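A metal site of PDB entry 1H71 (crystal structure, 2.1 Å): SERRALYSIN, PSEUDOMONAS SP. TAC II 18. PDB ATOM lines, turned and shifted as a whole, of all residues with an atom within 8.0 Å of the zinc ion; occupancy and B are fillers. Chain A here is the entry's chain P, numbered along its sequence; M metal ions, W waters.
Merely in contact with the zinc ion: Glu 170 (3.9 Å) and Tyr 209 (3.0 Å).
Of the 18 residues printed, 5 come within 4 Å of the zinc ion.
The zinc ion is bound by NE2 of His 173, water W1, NE2 of His 179 and NE2 of His 169.
The backbone NH (N) of Ala 132 is in hydrogen-bond range of the side-chain carboxylate (OE1) of Glu 170 (3.2 Å).
O of Val 206 lies within hydrogen-bond range of ND1 of His 169 (2.7 Å).
ND1 of His 179 sits at hydrogen-bond distance from O of Tyr 183, at 2.9 Å.
NE2 of His 179 sits close to OH of Tyr 209 (3.4 Å).
A ring nitrogen (ND1) of His 173 is in hydrogen-bond range of the backbone carbonyl oxygen (O) of Leu 177, at 2.8 Å.
Water W1 lies within hydrogen-bond range of OE2 of Glu 170 (2.6 Å) and OH of Tyr 209 (3.1 Å).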
ATOM      1  N   ALA A 130     -27.865  -5.510  -0.546  1.00  0.00           N
ATOM      2  CA  ALA A 130     -26.660  -4.699  -0.745  1.00  0.00           C
ATOM      3  C   ALA A 130     -25.505  -5.607  -1.199  1.00  0.00           C
ATOM      4  O   ALA A 130     -25.537  -6.833  -1.048  1.00  0.00           O
ATOM      5  CB  ALA A 130     -26.387  -3.895   0.519  1.00  0.00           C
ATOM      6  N   PHE A 131     -24.433  -5.059  -1.768  1.00  0.00           N
ATOM      7  CA  PHE A 131     -23.347  -5.939  -2.191  1.00  0.00           C
ATOM      8  C   PHE A 131     -22.121  -5.057  -2.357  1.00  0.00           C
ATOM      9  O   PHE A 131     -22.290  -3.826  -2.364  1.00  0.00           O
ATOM     10  CB  PHE A 131     -23.707  -6.858  -3.382  1.00  0.00           C
ATOM     11  CG  PHE A 131     -23.893  -6.065  -4.672  1.00  0.00           C
ATOM     12  CD1 PHE A 131     -22.839  -5.781  -5.488  1.00  0.00           C
ATOM     13  CD2 PHE A 131     -25.172  -5.631  -5.033  1.00  0.00           C
ATOM     14  CE1 PHE A 131     -23.046  -5.053  -6.682  1.00  0.00           C
ATOM     15  CE2 PHE A 131     -25.378  -4.879  -6.177  1.00  0.00           C
ATOM     16  CZ  PHE A 131     -24.297  -4.582  -6.990  1.00  0.00           C
ATOM     17  N   ALA A 132     -20.940  -5.633  -2.336  1.00  0.00           N
ATOM     18  CA  ALA A 132     -19.708  -4.819  -2.459  1.00  0.00           C
ATOM     19  C   ALA A 132     -18.634  -5.713  -3.105  1.00  0.00           C
ATOM     20  O   ALA A 132     -18.823  -6.912  -3.221  1.00  0.00           O
ATOM     21  CB  ALA A 132     -19.177  -4.355  -1.097  1.00  0.00           C
ATOM     22  N   TYR A 162     -30.758  -2.180  11.278  1.00  0.00           N
ATOM     23  CA  TYR A 162     -30.126  -2.971  10.225  1.00  0.00           C
ATOM     24  C   TYR A 162     -29.598  -2.178   9.044  1.00  0.00           C
ATOM     25  O   TYR A 162     -28.643  -2.617   8.385  1.00  0.00           O
ATOM     26  CB  TYR A 162     -31.079  -4.079   9.763  1.00  0.00           C
ATOM     27  CG  TYR A 162     -30.378  -5.106   8.904  1.00  0.00           C
ATOM     28  CD1 TYR A 162     -29.299  -5.792   9.481  1.00  0.00           C
ATOM     29  CD2 TYR A 162     -30.727  -5.391   7.599  1.00  0.00           C
ATOM     30  CE1 TYR A 162     -28.609  -6.761   8.733  1.00  0.00           C
ATOM     31  CE2 TYR A 162     -30.067  -6.349   6.847  1.00  0.00           C
ATOM     32  CZ  TYR A 162     -29.017  -7.035   7.439  1.00  0.00           C
ATOM     33  OH  TYR A 162     -28.334  -8.029   6.792  1.00  0.00           O
ATOM     34  N   THR A 166     -25.860  -2.706   7.847  1.00  0.00           N
ATOM     35  CA  THR A 166     -25.569  -3.028   6.424  1.00  0.00           C
ATOM     36  C   THR A 166     -24.439  -2.173   5.889  1.00  0.00           C
ATOM     37  O   THR A 166     -23.494  -2.646   5.232  1.00  0.00           O
ATOM     38  CB  THR A 166     -26.879  -2.851   5.606  1.00  0.00           C
ATOM     39  OG1 THR A 166     -27.736  -3.929   6.044  1.00  0.00           O
ATOM     40  CG2 THR A 166     -26.621  -3.038   4.094  1.00  0.00           C
ATOM     41  N   HIS A 169     -21.103  -3.423   7.392  1.00  0.00           N
ATOM     42  CA  HIS A 169     -20.818  -4.727   6.815  1.00  0.00           C
ATOM     43  C   HIS A 169     -20.277  -4.595   5.408  1.00  0.00           C
ATOM     44  O   HIS A 169     -19.270  -5.241   5.131  1.00  0.00           O
ATOM     45  CB  HIS A 169     -22.175  -5.462   6.883  1.00  0.00           C
ATOM     46  CG  HIS A 169     -22.200  -6.810   6.236  1.00  0.00           C
ATOM     47  ND1 HIS A 169     -22.358  -8.021   6.857  1.00  0.00           N
ATOM     48  CD2 HIS A 169     -22.060  -7.081   4.873  1.00  0.00           C
ATOM     49  CE1 HIS A 169     -22.347  -9.062   6.005  1.00  0.00           C
ATOM     50  NE2 HIS A 169     -22.183  -8.445   4.876  1.00  0.00           N
ATOM     51  N   GLU A 170     -20.936  -3.864   4.469  1.00  0.00           N
ATOM     52  CA  GLU A 170     -20.424  -3.756   3.094  1.00  0.00           C
ATOM     53  C   GLU A 170     -19.085  -3.052   3.032  1.00  0.00           C
ATOM     54  O   GLU A 170     -18.234  -3.486   2.252  1.00  0.00           O
ATOM     55  CB  GLU A 170     -21.413  -3.009   2.133  1.00  0.00           C
ATOM     56  CG  GLU A 170     -22.782  -3.729   2.051  1.00  0.00           C
ATOM     57  CD  GLU A 170     -22.681  -5.179   1.581  1.00  0.00           C
ATOM     58  OE1 GLU A 170     -21.776  -5.541   0.802  1.00  0.00           O
ATOM     59  OE2 GLU A 170     -23.491  -6.054   1.945  1.00  0.00           O
ATOM     60  N   GLY A 172     -16.879  -3.343   5.351  1.00  0.00           N
ATOM     61  CA  GLY A 172     -15.951  -4.431   5.770  1.00  0.00           C
ATOM     62  C   GLY A 172     -15.561  -5.250   4.507  1.00  0.00           C
ATOM     63  O   GLY A 172     -14.371  -5.577   4.429  1.00  0.00           O
ATOM     64  N   HIS A 173     -16.480  -5.616   3.604  1.00  0.00           N
ATOM     65  CA  HIS A 173     -16.056  -6.340   2.390  1.00  0.00           C
ATOM     66  C   HIS A 173     -15.119  -5.456   1.539  1.00  0.00           C
ATOM     67  O   HIS A 173     -14.149  -5.986   0.975  1.00  0.00           O
ATOM     68  CB  HIS A 173     -17.205  -6.564   1.392  1.00  0.00           C
ATOM     69  CG  HIS A 173     -18.120  -7.607   1.889  1.00  0.00           C
ATOM     70  ND1 HIS A 173     -17.746  -8.898   2.240  1.00  0.00           N
ATOM     71  CD2 HIS A 173     -19.490  -7.525   2.007  1.00  0.00           C
ATOM     72  CE1 HIS A 173     -18.753  -9.619   2.629  1.00  0.00           C
ATOM     73  NE2 HIS A 173     -19.785  -8.817   2.385  1.00  0.00           N
ATOM     74  N   LEU A 177     -12.729  -8.053   3.953  1.00  0.00           N
ATOM     75  CA  LEU A 177     -13.283  -9.091   4.812  1.00  0.00           C
ATOM     76  C   LEU A 177     -14.306  -9.904   4.036  1.00  0.00           C
ATOM     77  O   LEU A 177     -15.160  -9.379   3.290  1.00  0.00           O
ATOM     78  CB  LEU A 177     -13.922  -8.561   6.117  1.00  0.00           C
ATOM     79  CG  LEU A 177     -13.114  -7.641   7.040  1.00  0.00           C
ATOM     80  CD1 LEU A 177     -13.888  -7.377   8.376  1.00  0.00           C
ATOM     81  CD2 LEU A 177     -11.804  -8.353   7.379  1.00  0.00           C
ATOM     82  N   SER A 178     -14.362 -11.204   4.251  1.00  0.00           N
ATOM     83  CA  SER A 178     -15.380 -12.056   3.660  1.00  0.00           C
ATOM     84  C   SER A 178     -16.465 -12.369   4.672  1.00  0.00           C
ATOM     85  O   SER A 178     -16.247 -12.100   5.859  1.00  0.00           O
ATOM     86  CB  SER A 178     -14.746 -13.436   3.348  1.00  0.00           C
ATOM     87  OG  SER A 178     -13.657 -13.216   2.464  1.00  0.00           O
ATOM     88  N   HIS A 179     -17.570 -12.998   4.277  1.00  0.00           N
ATOM     89  CA  HIS A 179     -18.501 -13.594   5.218  1.00  0.00           C
ATOM     90  C   HIS A 179     -17.721 -14.679   5.953  1.00  0.00           C
ATOM     91  O   HIS A 179     -16.844 -15.294   5.351  1.00  0.00           O
ATOM     92  CB  HIS A 179     -19.596 -14.390   4.442  1.00  0.00           C
ATOM     93  CG  HIS A 179     -20.448 -13.369   3.749  1.00  0.00           C
ATOM     94  ND1 HIS A 179     -20.943 -13.572   2.493  1.00  0.00           N
ATOM     95  CD2 HIS A 179     -20.894 -12.158   4.118  1.00  0.00           C
ATOM     96  CE1 HIS A 179     -21.635 -12.558   2.026  1.00  0.00           C
ATOM     97  NE2 HIS A 179     -21.621 -11.721   3.007  1.00  0.00           N
ATOM     98  N   PRO A 180     -18.134 -15.041   7.158  1.00  0.00           N
ATOM     99  CA  PRO A 180     -17.458 -16.058   7.942  1.00  0.00           C
ATOM    100  C   PRO A 180     -17.533 -17.427   7.297  1.00  0.00           C
ATOM    101  O   PRO A 180     -16.851 -18.337   7.804  1.00  0.00           O
ATOM    102  CB  PRO A 180     -18.274 -16.093   9.256  1.00  0.00           C
ATOM    103  CG  PRO A 180     -18.832 -14.723   9.374  1.00  0.00           C
ATOM    104  CD  PRO A 180     -19.171 -14.344   7.961  1.00  0.00           C
ATOM    105  N   TYR A 183     -21.070 -18.600   1.852  1.00  0.00           N
ATOM    106  CA  TYR A 183     -22.518 -18.418   1.676  1.00  0.00           C
ATOM    107  C   TYR A 183     -22.745 -16.941   1.237  1.00  0.00           C
ATOM    108  O   TYR A 183     -21.810 -16.166   1.647  1.00  0.00           O
ATOM    109  CB  TYR A 183     -23.240 -18.817   2.940  1.00  0.00           C
ATOM    110  CG  TYR A 183     -22.889 -18.094   4.218  1.00  0.00           C
ATOM    111  CD1 TYR A 183     -22.370 -18.773   5.317  1.00  0.00           C
ATOM    112  CD2 TYR A 183     -23.111 -16.732   4.335  1.00  0.00           C
ATOM    113  CE1 TYR A 183     -22.048 -18.102   6.488  1.00  0.00           C
ATOM    114  CE2 TYR A 183     -22.792 -16.058   5.492  1.00  0.00           C
ATOM    115  CZ  TYR A 183     -22.264 -16.762   6.576  1.00  0.00           C
ATOM    116  OH  TYR A 183     -22.016 -16.026   7.728  1.00  0.00           O
ATOM    117  N   VAL A 206     -20.045  -8.444  12.525  1.00  0.00           N
ATOM    118  CA  VAL A 206     -21.095  -7.815  11.719  1.00  0.00           C
ATOM    119  C   VAL A 206     -21.036  -8.426  10.289  1.00  0.00           C
ATOM    120  O   VAL A 206     -21.940  -8.123   9.525  1.00  0.00           O
ATOM    121  CB  VAL A 206     -21.051  -6.294  11.636  1.00  0.00           C
ATOM    122  CG1 VAL A 206     -21.101  -5.597  13.015  1.00  0.00           C
ATOM    123  CG2 VAL A 206     -19.804  -5.839  10.851  1.00  0.00           C
ATOM    124  N   MET A 207     -20.100  -9.290   9.962  1.00  0.00           N
ATOM    125  CA  MET A 207     -19.976  -9.914   8.639  1.00  0.00           C
ATOM    126  C   MET A 207     -20.918 -11.106   8.523  1.00  0.00           C
ATOM    127  O   MET A 207     -21.140 -11.712   7.466  1.00  0.00           O
ATOM    128  CB  MET A 207     -18.525 -10.315   8.327  1.00  0.00           C
ATOM    129  CG  MET A 207     -17.494  -9.139   8.327  1.00  0.00           C
ATOM    130  SD  MET A 207     -18.080  -7.707   7.406  1.00  0.00           S
ATOM    131  CE  MET A 207     -18.089  -8.376   5.720  1.00  0.00           C
ATOM    132  N   SER A 208     -21.334 -11.670   9.670  1.00  0.00           N
ATOM    133  CA  SER A 208     -22.255 -12.783   9.646  1.00  0.00           C
ATOM    134  C   SER A 208     -23.673 -12.369   9.281  1.00  0.00           C
ATOM    135  O   SER A 208     -24.066 -11.248   9.564  1.00  0.00           O
ATOM    136  CB  SER A 208     -22.393 -13.244  11.146  1.00  0.00           C
ATOM    137  OG  SER A 208     -23.162 -14.439  11.192  1.00  0.00           O
ATOM    138  N   TYR A 209     -24.470 -13.294   8.794  1.00  0.00           N
ATOM    139  CA  TYR A 209     -25.860 -13.145   8.491  1.00  0.00           C
ATOM    140  C   TYR A 209     -26.789 -13.762   9.524  1.00  0.00           C
ATOM    141  O   TYR A 209     -27.999 -13.623   9.478  1.00  0.00           O
ATOM    142  CB  TYR A 209     -26.124 -13.812   7.127  1.00  0.00           C
ATOM    143  CG  TYR A 209     -25.726 -12.866   5.977  1.00  0.00           C
ATOM    144  CD1 TYR A 209     -26.064 -11.516   6.017  1.00  0.00           C
ATOM    145  CD2 TYR A 209     -25.051 -13.305   4.868  1.00  0.00           C
ATOM    146  CE1 TYR A 209     -25.716 -10.650   4.989  1.00  0.00           C
ATOM    147  CE2 TYR A 209     -24.706 -12.474   3.826  1.00  0.00           C
ATOM    148  CZ  TYR A 209     -25.032 -11.145   3.889  1.00  0.00           C
ATOM    149  OH  TYR A 209     -24.731 -10.261   2.900  1.00  0.00           O
HETATM  150 ZN    ZN M   1     -21.882  -9.472   2.860  1.00  0.00          ZN
HETATM  151  O   HOH W   1     -22.962  -8.446   1.169  1.00  0.00           O
